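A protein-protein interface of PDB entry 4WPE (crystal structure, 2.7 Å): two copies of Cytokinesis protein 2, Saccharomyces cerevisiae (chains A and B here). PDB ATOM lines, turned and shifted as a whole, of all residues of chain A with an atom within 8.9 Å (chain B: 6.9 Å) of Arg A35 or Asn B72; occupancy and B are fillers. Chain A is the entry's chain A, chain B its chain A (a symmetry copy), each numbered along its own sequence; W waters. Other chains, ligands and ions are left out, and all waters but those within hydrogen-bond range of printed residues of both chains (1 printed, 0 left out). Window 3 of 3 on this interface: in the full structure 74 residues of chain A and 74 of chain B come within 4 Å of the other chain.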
ATOM      1  N   LEU A  27     -21.892 -29.944   2.529  1.00  0.00           N
ATOM      2  CA  LEU A  27     -21.551 -28.561   2.840  1.00  0.00           C
ATOM      3  C   LEU A  27     -21.372 -28.378   4.343  1.00  0.00           C
ATOM      4  O   LEU A  27     -20.517 -27.612   4.789  1.00  0.00           O
ATOM      5  CB  LEU A  27     -22.622 -27.604   2.315  1.00  0.00           C
ATOM      6  CG  LEU A  27     -22.668 -27.431   0.796  1.00  0.00           C
ATOM      7  CD1 LEU A  27     -23.751 -26.442   0.397  1.00  0.00           C
ATOM      8  CD2 LEU A  27     -21.314 -26.982   0.280  1.00  0.00           C
ATOM      9  N   GLY A  28     -22.178 -29.096   5.118  1.00  0.00           N
ATOM     10  CA  GLY A  28     -22.076 -29.053   6.564  1.00  0.00           C
ATOM     11  C   GLY A  28     -20.789 -29.693   7.045  1.00  0.00           C
ATOM     12  O   GLY A  28     -20.132 -29.180   7.953  1.00  0.00           O
ATOM     13  N   HIS A  29     -20.425 -30.810   6.421  1.00  0.00           N
ATOM     14  CA  HIS A  29     -19.237 -31.560   6.815  1.00  0.00           C
ATOM     15  C   HIS A  29     -17.941 -30.792   6.548  1.00  0.00           C
ATOM     16  O   HIS A  29     -17.058 -30.733   7.407  1.00  0.00           O
ATOM     17  CB  HIS A  29     -19.193 -32.908   6.094  1.00  0.00           C
ATOM     18  CG  HIS A  29     -18.033 -33.760   6.481  1.00  0.00           C
ATOM     19  ND1 HIS A  29     -17.704 -34.021   7.807  1.00  0.00           N
ATOM     20  CD2 HIS A  29     -17.108 -34.416   5.747  1.00  0.00           C
ATOM     21  CE1 HIS A  29     -16.645 -34.790   7.852  1.00  0.00           C
ATOM     22  NE2 HIS A  29     -16.255 -35.052   6.609  1.00  0.00           N
ATOM     23  N   ILE A  30     -17.827 -30.216   5.355  1.00  0.00           N
ATOM     24  CA  ILE A  30     -16.640 -29.456   4.983  1.00  0.00           C
ATOM     25  C   ILE A  30     -16.500 -28.218   5.869  1.00  0.00           C
ATOM     26  O   ILE A  30     -15.401 -27.875   6.307  1.00  0.00           O
ATOM     27  CB  ILE A  30     -16.676 -29.047   3.487  1.00  0.00           C
ATOM     28  CG1 ILE A  30     -16.056 -30.142   2.617  1.00  0.00           C
ATOM     29  CG2 ILE A  30     -15.925 -27.744   3.249  1.00  0.00           C
ATOM     30  CD1 ILE A  30     -16.917 -31.375   2.446  1.00  0.00           C
ATOM     31  N   SER A  31     -17.627 -27.570   6.149  1.00  0.00           N
ATOM     32  CA  SER A  31     -17.647 -26.360   6.964  1.00  0.00           C
ATOM     33  C   SER A  31     -17.215 -26.625   8.404  1.00  0.00           C
ATOM     34  O   SER A  31     -16.471 -25.841   8.991  1.00  0.00           O
ATOM     35  CB  SER A  31     -19.044 -25.736   6.951  1.00  0.00           C
ATOM     36  OG  SER A  31     -19.225 -24.863   8.050  1.00  0.00           O
ATOM     37  N   GLN A  32     -17.685 -27.731   8.972  1.00  0.00           N
ATOM     38  CA  GLN A  32     -17.350 -28.054  10.352  1.00  0.00           C
ATOM     39  C   GLN A  32     -15.894 -28.495  10.446  1.00  0.00           C
ATOM     40  O   GLN A  32     -15.263 -28.367  11.496  1.00  0.00           O
ATOM     41  CB  GLN A  32     -18.280 -29.139  10.905  1.00  0.00           C
ATOM     42  CG  GLN A  32     -17.790 -30.566  10.697  1.00  0.00           C
ATOM     43  CD  GLN A  32     -18.423 -31.547  11.669  1.00  0.00           C
ATOM     44  OE1 GLN A  32     -19.298 -31.182  12.456  1.00  0.00           O
ATOM     45  NE2 GLN A  32     -17.973 -32.797  11.626  1.00  0.00           N
ATOM     46  N   GLY A  33     -15.365 -29.005   9.338  1.00  0.00           N
ATOM     47  CA  GLY A  33     -13.986 -29.449   9.285  1.00  0.00           C
ATOM     48  C   GLY A  33     -13.039 -28.269   9.242  1.00  0.00           C
ATOM     49  O   GLY A  33     -11.890 -28.355   9.678  1.00  0.00           O
ATOM     50  N   ILE A  34     -13.529 -27.157   8.712  1.00  0.00           N
ATOM     51  CA  ILE A  34     -12.734 -25.942   8.630  1.00  0.00           C
ATOM     52  C   ILE A  34     -12.576 -25.315  10.015  1.00  0.00           C
ATOM     53  O   ILE A  34     -11.476 -24.920  10.404  1.00  0.00           O
ATOM     54  CB  ILE A  34     -13.364 -24.937   7.650  1.00  0.00           C
ATOM     55  CG1 ILE A  34     -13.199 -25.445   6.218  1.00  0.00           C
ATOM     56  CG2 ILE A  34     -12.711 -23.572   7.775  1.00  0.00           C
ATOM     57  CD1 ILE A  34     -14.027 -24.696   5.212  1.00  0.00           C
ATOM     58  N   ARG A  35     -13.673 -25.242  10.764  1.00  0.00           N
ATOM     59  CA  ARG A  35     -13.637 -24.726  12.131  1.00  0.00           C
ATOM     60  C   ARG A  35     -12.838 -25.652  13.034  1.00  0.00           C
ATOM     61  O   ARG A  35     -12.236 -25.216  14.012  1.00  0.00           O
ATOM     62  CB  ARG A  35     -15.051 -24.552  12.690  1.00  0.00           C
ATOM     63  CG  ARG A  35     -15.907 -23.552  11.936  1.00  0.00           C
ATOM     64  CD  ARG A  35     -17.385 -23.786  12.206  1.00  0.00           C
ATOM     65  NE  ARG A  35     -18.226 -22.803  11.530  1.00  0.00           N
ATOM     66  CZ  ARG A  35     -19.472 -22.511  11.889  1.00  0.00           C
ATOM     67  NH1 ARG A  35     -20.030 -23.129  12.921  1.00  0.00           N
ATOM     68  NH2 ARG A  35     -20.161 -21.601  11.213  1.00  0.00           N
ATOM     69  N   SER A  36     -12.838 -26.936  12.695  1.00  0.00           N
ATOM     70  CA  SER A  36     -12.128 -27.944  13.470  1.00  0.00           C
ATOM     71  C   SER A  36     -10.616 -27.735  13.399  1.00  0.00           C
ATOM     72  O   SER A  36      -9.874 -28.212  14.260  1.00  0.00           O
ATOM     73  CB  SER A  36     -12.497 -29.344  12.978  1.00  0.00           C
ATOM     74  OG  SER A  36     -11.655 -30.328  13.550  1.00  0.00           O
ATOM     75  N   CYS A  37     -10.161 -27.020  12.373  1.00  0.00           N
ATOM     76  CA  CYS A  37      -8.745 -26.697  12.238  1.00  0.00           C
ATOM     77  C   CYS A  37      -8.293 -25.758  13.350  1.00  0.00           C
ATOM     78  O   CYS A  37      -7.142 -25.807  13.784  1.00  0.00           O
ATOM     79  CB  CYS A  37      -8.456 -26.066  10.873  1.00  0.00           C
ATOM     80  SG  CYS A  37      -8.535 -27.202   9.467  1.00  0.00           S
ATOM     81  N   ASP A  38      -9.206 -24.909  13.814  1.00  0.00           N
ATOM     82  CA  ASP A  38      -8.902 -23.951  14.872  1.00  0.00           C
ATOM     83  C   ASP A  38      -8.455 -24.649  16.156  1.00  0.00           C
ATOM     84  O   ASP A  38      -7.786 -24.051  16.996  1.00  0.00           O
ATOM     85  CB  ASP A  38     -10.116 -23.064  15.160  1.00  0.00           C
ATOM     86  CG  ASP A  38     -10.435 -22.123  14.016  1.00  0.00           C
ATOM     87  OD1 ASP A  38      -9.494 -21.533  13.444  1.00  0.00           O
ATOM     88  OD2 ASP A  38     -11.629 -21.968  13.689  1.00  0.00           O
ATOM     89  N   SER A  39      -8.836 -25.913  16.302  1.00  0.00           N
ATOM     90  CA  SER A  39      -8.417 -26.702  17.449  1.00  0.00           C
ATOM     91  C   SER A  39      -6.905 -26.889  17.432  1.00  0.00           C
ATOM     92  O   SER A  39      -6.233 -26.706  18.449  1.00  0.00           O
ATOM     93  CB  SER A  39      -9.117 -28.063  17.454  1.00  0.00           C
ATOM     94  OG  SER A  39     -10.528 -27.923  17.445  1.00  0.00           O
ATOM     95  N   MET A  40      -6.373 -27.248  16.269  1.00  0.00           N
ATOM     96  CA  MET A  40      -4.943 -27.490  16.129  1.00  0.00           C
ATOM     97  C   MET A  40      -4.159 -26.191  15.955  1.00  0.00           C
ATOM     98  O   MET A  40      -3.047 -26.062  16.472  1.00  0.00           O
ATOM     99  CB  MET A  40      -4.673 -28.437  14.956  1.00  0.00           C
ATOM    100  CG  MET A  40      -4.878 -29.908  15.299  1.00  0.00           C
ATOM    101  SD  MET A  40      -3.791 -30.463  16.830  1.00  0.00           S
ATOM    102  CE  MET A  40      -4.441 -32.289  17.042  1.00  0.00           C
ATOM    103  N   ILE A  41      -4.742 -25.235  15.234  1.00  0.00           N
ATOM    104  CA  ILE A  41      -4.121 -23.927  15.047  1.00  0.00           C
ATOM    105  C   ILE A  41      -3.792 -23.278  16.388  1.00  0.00           C
ATOM    106  O   ILE A  41      -2.680 -22.794  16.597  1.00  0.00           O
ATOM    107  CB  ILE A  41      -5.029 -22.975  14.243  1.00  0.00           C
ATOM    108  CG1 ILE A  41      -5.153 -23.446  12.795  1.00  0.00           C
ATOM    109  CG2 ILE A  41      -4.473 -21.561  14.266  1.00  0.00           C
ATOM    110  CD1 ILE A  41      -6.277 -22.763  12.032  1.00  0.00           C
ATOM    111  N   LEU A  42      -4.758 -23.279  17.301  1.00  0.00           N
ATOM    112  CA  LEU A  42      -4.550 -22.702  18.623  1.00  0.00           C
ATOM    113  C   LEU A  42      -3.542 -23.520  19.418  1.00  0.00           C
ATOM    114  O   LEU A  42      -2.696 -22.963  20.117  1.00  0.00           O
ATOM    115  CB  LEU A  42      -5.869 -22.608  19.391  1.00  0.00           C
ATOM    116  CG  LEU A  42      -5.795 -21.854  20.724  1.00  0.00           C
ATOM    117  CD1 LEU A  42      -5.595 -20.362  20.494  1.00  0.00           C
ATOM    118  CD2 LEU A  42      -7.033 -22.111  21.569  1.00  0.00           C
ATOM    119  N   ALA A 115      -5.927 -22.684   6.432  1.00  0.00           N
ATOM    120  CA  ALA A 115      -7.305 -22.776   6.905  1.00  0.00           C
ATOM    121  C   ALA A 115      -8.131 -21.596   6.414  1.00  0.00           C
ATOM    122  O   ALA A 115      -9.289 -21.754   6.047  1.00  0.00           O
ATOM    123  CB  ALA A 115      -7.345 -22.850   8.423  1.00  0.00           C
ATOM    124  N   LEU A 118      -8.990 -22.268   2.787  1.00  0.00           N
ATOM    125  CA  LEU A 118     -10.060 -23.247   2.651  1.00  0.00           C
ATOM    126  C   LEU A 118     -11.403 -22.560   2.842  1.00  0.00           C
ATOM    127  O   LEU A 118     -12.334 -22.766   2.062  1.00  0.00           O
ATOM    128  CB  LEU A 118      -9.905 -24.382   3.662  1.00  0.00           C
ATOM    129  CG  LEU A 118      -8.936 -25.511   3.314  1.00  0.00           C
ATOM    130  CD1 LEU A 118      -9.255 -26.739   4.152  1.00  0.00           C
ATOM    131  CD2 LEU A 118      -8.991 -25.838   1.832  1.00  0.00           C
ATOM    132  N   GLN A 119     -11.485 -21.737   3.883  1.00  0.00           N
ATOM    133  CA  GLN A 119     -12.690 -20.969   4.181  1.00  0.00           C
ATOM    134  C   GLN A 119     -13.105 -20.086   3.004  1.00  0.00           C
ATOM    135  O   GLN A 119     -14.287 -19.991   2.677  1.00  0.00           O
ATOM    136  CB  GLN A 119     -12.474 -20.113   5.429  1.00  0.00           C
ATOM    137  CG  GLN A 119     -13.633 -19.193   5.767  1.00  0.00           C
ATOM    138  CD  GLN A 119     -14.915 -19.948   6.039  1.00  0.00           C
ATOM    139  OE1 GLN A 119     -14.900 -21.015   6.654  1.00  0.00           O
ATOM    140  NE2 GLN A 119     -16.036 -19.401   5.581  1.00  0.00           N
ATOM    141  N   TYR A 122     -14.490 -22.315   0.284  1.00  0.00           N
ATOM    142  CA  TYR A 122     -15.768 -22.859   0.727  1.00  0.00           C
ATOM    143  C   TYR A 122     -16.890 -21.835   0.585  1.00  0.00           C
ATOM    144  O   TYR A 122     -17.995 -22.171   0.158  1.00  0.00           O
ATOM    145  CB  TYR A 122     -15.687 -23.336   2.179  1.00  0.00           C
ATOM    146  CG  TYR A 122     -17.045 -23.631   2.768  1.00  0.00           C
ATOM    147  CD1 TYR A 122     -17.713 -24.808   2.461  1.00  0.00           C
ATOM    148  CD2 TYR A 122     -17.671 -22.723   3.613  1.00  0.00           C
ATOM    149  CE1 TYR A 122     -18.961 -25.082   2.987  1.00  0.00           C
ATOM    150  CE2 TYR A 122     -18.922 -22.986   4.142  1.00  0.00           C
ATOM    151  CZ  TYR A 122     -19.562 -24.168   3.826  1.00  0.00           C
ATOM    152  OH  TYR A 122     -20.805 -24.438   4.353  1.00  0.00           O
ATOM    153  N   ARG A 226      -7.683 -31.014   2.910  1.00  0.00           N
ATOM    154  CA  ARG A 226      -7.727 -30.645   4.320  1.00  0.00           C
ATOM    155  C   ARG A 226      -7.153 -31.753   5.205  1.00  0.00           C
ATOM    156  O   ARG A 226      -6.315 -31.495   6.071  1.00  0.00           O
ATOM    157  CB  ARG A 226      -9.157 -30.324   4.744  1.00  0.00           C
ATOM    158  CG  ARG A 226      -9.299 -29.999   6.220  1.00  0.00           C
ATOM    159  CD  ARG A 226     -10.762 -29.953   6.637  1.00  0.00           C
ATOM    160  NE  ARG A 226     -10.904 -30.099   8.079  1.00  0.00           N
ATOM    161  CZ  ARG A 226     -11.147 -31.252   8.693  1.00  0.00           C
ATOM    162  NH1 ARG A 226     -11.291 -32.365   7.985  1.00  0.00           N
ATOM    163  NH2 ARG A 226     -11.253 -31.291  10.014  1.00  0.00           N
ATOM    164  N   LEU A 230      -3.337 -31.517   7.148  1.00  0.00           N
ATOM    165  CA  LEU A 230      -3.268 -31.701   8.597  1.00  0.00           C
ATOM    166  C   LEU A 230      -2.486 -32.960   8.939  1.00  0.00           C
ATOM    167  O   LEU A 230      -1.770 -33.007   9.936  1.00  0.00           O
ATOM    168  CB  LEU A 230      -4.668 -31.779   9.208  1.00  0.00           C
ATOM    169  CG  LEU A 230      -5.536 -30.520   9.165  1.00  0.00           C
ATOM    170  CD1 LEU A 230      -6.860 -30.762   9.873  1.00  0.00           C
ATOM    171  CD2 LEU A 230      -4.805 -29.341   9.786  1.00  0.00           C
ATOM    172  N   LYS B  67     -11.483 -29.433  25.033  1.00  0.00           N
ATOM    173  CA  LYS B  67     -12.741 -28.721  24.847  1.00  0.00           C
ATOM    174  C   LYS B  67     -12.960 -28.367  23.381  1.00  0.00           C
ATOM    175  O   LYS B  67     -14.092 -28.364  22.898  1.00  0.00           O
ATOM    176  CB  LYS B  67     -12.773 -27.453  25.707  1.00  0.00           C
ATOM    177  N   ASP B  68     -11.875 -28.073  22.672  1.00  0.00           N
ATOM    178  CA  ASP B  68     -11.972 -27.705  21.262  1.00  0.00           C
ATOM    179  C   ASP B  68     -12.327 -28.901  20.386  1.00  0.00           C
ATOM    180  O   ASP B  68     -13.108 -28.775  19.446  1.00  0.00           O
ATOM    181  CB  ASP B  68     -10.669 -27.067  20.784  1.00  0.00           C
ATOM    182  CG  ASP B  68     -10.518 -25.636  21.255  1.00  0.00           C
ATOM    183  OD1 ASP B  68     -11.179 -25.272  22.251  1.00  0.00           O
ATOM    184  OD2 ASP B  68      -9.743 -24.878  20.634  1.00  0.00           O
ATOM    185  N   ILE B  69     -11.750 -30.058  20.692  1.00  0.00           N
ATOM    186  CA  ILE B  69     -12.075 -31.280  19.966  1.00  0.00           C
ATOM    187  C   ILE B  69     -13.560 -31.607  20.106  1.00  0.00           C
ATOM    188  O   ILE B  69     -14.229 -31.937  19.124  1.00  0.00           O
ATOM    189  CB  ILE B  69     -11.229 -32.471  20.459  1.00  0.00           C
ATOM    190  CG1 ILE B  69      -9.780 -32.319  19.991  1.00  0.00           C
ATOM    191  CG2 ILE B  69     -11.801 -33.787  19.958  1.00  0.00           C
ATOM    192  CD1 ILE B  69      -8.851 -33.387  20.524  1.00  0.00           C
ATOM    193  N   GLY B  70     -14.073 -31.492  21.327  1.00  0.00           N
ATOM    194  CA  GLY B  70     -15.475 -31.751  21.600  1.00  0.00           C
ATOM    195  C   GLY B  70     -16.400 -30.731  20.961  1.00  0.00           C
ATOM    196  O   GLY B  70     -17.408 -31.093  20.350  1.00  0.00           O
ATOM    197  N   THR B  71     -16.060 -29.452  21.105  1.00  0.00           N
ATOM    198  CA  THR B  71     -16.839 -28.377  20.495  1.00  0.00           C
ATOM    199  C   THR B  71     -16.784 -28.471  18.975  1.00  0.00           C
ATOM    200  O   THR B  71     -17.785 -28.771  18.323  1.00  0.00           O
ATOM    201  CB  THR B  71     -16.336 -26.989  20.931  1.00  0.00           C
ATOM    202  OG1 THR B  71     -16.429 -26.870  22.356  1.00  0.00           O
ATOM    203  CG2 THR B  71     -17.164 -25.892  20.272  1.00  0.00           C
ATOM    204  N   ASN B  72     -15.606 -28.210  18.418  1.00  0.00           N
ATOM    205  CA  ASN B  72     -15.371 -28.405  16.996  1.00  0.00           C
ATOM    206  C   ASN B  72     -15.202 -29.884  16.690  1.00  0.00           C
ATOM    207  O   ASN B  72     -14.081 -30.383  16.596  1.00  0.00           O
ATOM    208  CB  ASN B  72     -14.134 -27.635  16.537  1.00  0.00           C
ATOM    209  CG  ASN B  72     -14.158 -26.187  16.971  1.00  0.00           C
ATOM    210  OD1 ASN B  72     -15.213 -25.552  16.999  1.00  0.00           O
ATOM    211  ND2 ASN B  72     -12.989 -25.654  17.319  1.00  0.00           N
ATOM    212  N   MET B  73     -16.320 -30.585  16.551  1.00  0.00           N
ATOM    213  CA  MET B  73     -16.292 -32.007  16.251  1.00  0.00           C
ATOM    214  C   MET B  73     -15.620 -32.267  14.911  1.00  0.00           C
ATOM    215  O   MET B  73     -15.677 -31.434  14.004  1.00  0.00           O
ATOM    216  CB  MET B  73     -17.708 -32.578  16.246  1.00  0.00           C
ATOM    217  CG  MET B  73     -18.385 -32.544  17.601  1.00  0.00           C
ATOM    218  SD  MET B  73     -20.180 -33.280  17.533  1.00  0.00           S
ATOM    219  CE  MET B  73     -21.031 -31.883  16.471  1.00  0.00           C
ATOM    220  N   ASP B  74     -14.972 -33.420  14.802  1.00  0.00           N
ATOM    221  CA  ASP B  74     -14.333 -33.826  13.559  1.00  0.00           C
ATOM    222  C   ASP B  74     -14.625 -35.299  13.302  1.00  0.00           C
ATOM    223  O   ASP B  74     -15.152 -35.993  14.171  1.00  0.00           O
ATOM    224  CB  ASP B  74     -12.830 -33.564  13.608  1.00  0.00           C
ATOM    225  CG  ASP B  74     -12.249 -33.254  12.242  1.00  0.00           C
ATOM    226  OD1 ASP B  74     -12.613 -33.945  11.266  1.00  0.00           O
ATOM    227  OD2 ASP B  74     -11.431 -32.315  12.142  1.00  0.00           O
ATOM    228  N   ASN B  79     -10.221 -37.449  13.529  1.00  0.00           N
ATOM    229  CA  ASN B  79     -10.683 -37.148  14.876  1.00  0.00           C
ATOM    230  C   ASN B  79     -10.010 -38.048  15.905  1.00  0.00           C
ATOM    231  O   ASN B  79      -9.673 -37.607  16.994  1.00  0.00           O
ATOM    232  CB  ASN B  79     -12.205 -37.269  14.964  1.00  0.00           C
ATOM    233  CG  ASN B  79     -12.752 -36.761  16.278  1.00  0.00           C
ATOM    234  OD1 ASN B  79     -13.260 -37.532  17.090  1.00  0.00           O
ATOM    235  ND2 ASN B  79     -12.640 -35.456  16.501  1.00  0.00           N
ATOM    236  N   PHE B  82      -6.665 -36.632  16.470  1.00  0.00           N
ATOM    237  CA  PHE B  82      -6.666 -35.444  17.316  1.00  0.00           C
ATOM    238  C   PHE B  82      -6.635 -35.861  18.779  1.00  0.00           C
ATOM    239  O   PHE B  82      -6.099 -35.149  19.628  1.00  0.00           O
ATOM    240  CB  PHE B  82      -7.892 -34.564  17.046  1.00  0.00           C
ATOM    241  CG  PHE B  82      -7.730 -33.619  15.881  1.00  0.00           C
ATOM    242  CD1 PHE B  82      -6.773 -33.846  14.906  1.00  0.00           C
ATOM    243  CD2 PHE B  82      -8.534 -32.494  15.772  1.00  0.00           C
ATOM    244  CE1 PHE B  82      -6.629 -32.975  13.839  1.00  0.00           C
ATOM    245  CE2 PHE B  82      -8.391 -31.620  14.708  1.00  0.00           C
ATOM    246  CZ  PHE B  82      -7.438 -31.861  13.742  1.00  0.00           C
HETATM  247  O   HOH W   1     -11.093 -30.407  16.193  1.00  0.00           O
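Of the 22 printed residues of chain A, 7 touch a printed residue of chain B.
Printed residues of chain A that touch a printed residue of chain B: Gln A32, Arg A35, Ser A36, Ser A39, Met A40, Leu A42 and Arg A226.
Hydrophobic or aromatic side chains of chain A that line the printed part of chain B: Met A40 and Leu A42.
Arg A35 touches one residue of chain B.
Of chain A, only Arg A35, Ser A36 and Ser A39 come within 4 Å of Asn B72.
No residue of chain A comes within 4 Å of Gly B70.
No residue of chain A comes within 4 Å of Thr B71.
Of the printed residues of chain B, Arg A226 touches Asp B74.
Of the printed residues of chain B, Ser A36 touches Asn B72, Met B73, Asp B74 and Phe B82.
His A29 touches none of the printed residues of chain B.
Tyr A122 touches none of the printed residues of chain B.
The nearest residue of chain B that does not touch Arg A35 is Met B73 (6.5 Å).
The nearest printed residue of chain A that does not touch Asp B68 is Asp A38 (4.2 Å).
Among the printed residues, pairs that only touch across the chains: Met A40 with Phe B82 (3.5 Å), Gln A32 with Met B73 (3.6 Å), Ser A36 with Asn B72 (3.7 Å), Ser A36 with Phe B82 (3.7 Å), Ser A36 with Met B73 (3.9 Å) and Leu A42 with Asp B68 (3.98 Å).
No position is printed for both chains.
Of the 11 pairs that touch across the chains among the printed residues, none has its exchanged pair printed and touching as well.
Water W1 lies within hydrogen-bond range of OG of Ser A36 (2.7 Å), OG of Ser A39 (2.8 Å) and O of Asn B72 (3.0 Å).
The side-chain amide nitrogen of Asn B72 is in hydrogen-bond range of the backbone carbonyl oxygen of Arg A35 (3.4 Å).
The side-chain hydroxyl of Ser A36 lies within hydrogen-bond range of the side-chain carboxylate of Asp B74 (2.4 Å).
The side-chain hydroxyl (OG) of Ser A39 is in hydrogen-bond range of the backbone carbonyl oxygen (O) of Asp B68.
The side-chain amide nitrogen of Asn B72 lies within hydrogen-bond range of the side-chain hydroxyl of Ser A39 (3.3 Å).
The guanidinium group (NH2) of Arg A226 is in salt-bridge range of the side-chain carboxylate (OD1) of Asp B74.
The guanidinium group (NE) of Arg A226 sits at hydrogen-bond distance from the backbone carbonyl oxygen (O) of Gly A33, 2.6 Å away.
The backbone carbonyl oxygen of Ser A36 sits at hydrogen-bond distance from the side-chain hydroxyl of Ser A39.
The backbone carbonyl oxygen of Asp B74 sits close to the side-chain amide nitrogen of Asn B79, at 3.5 Å.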
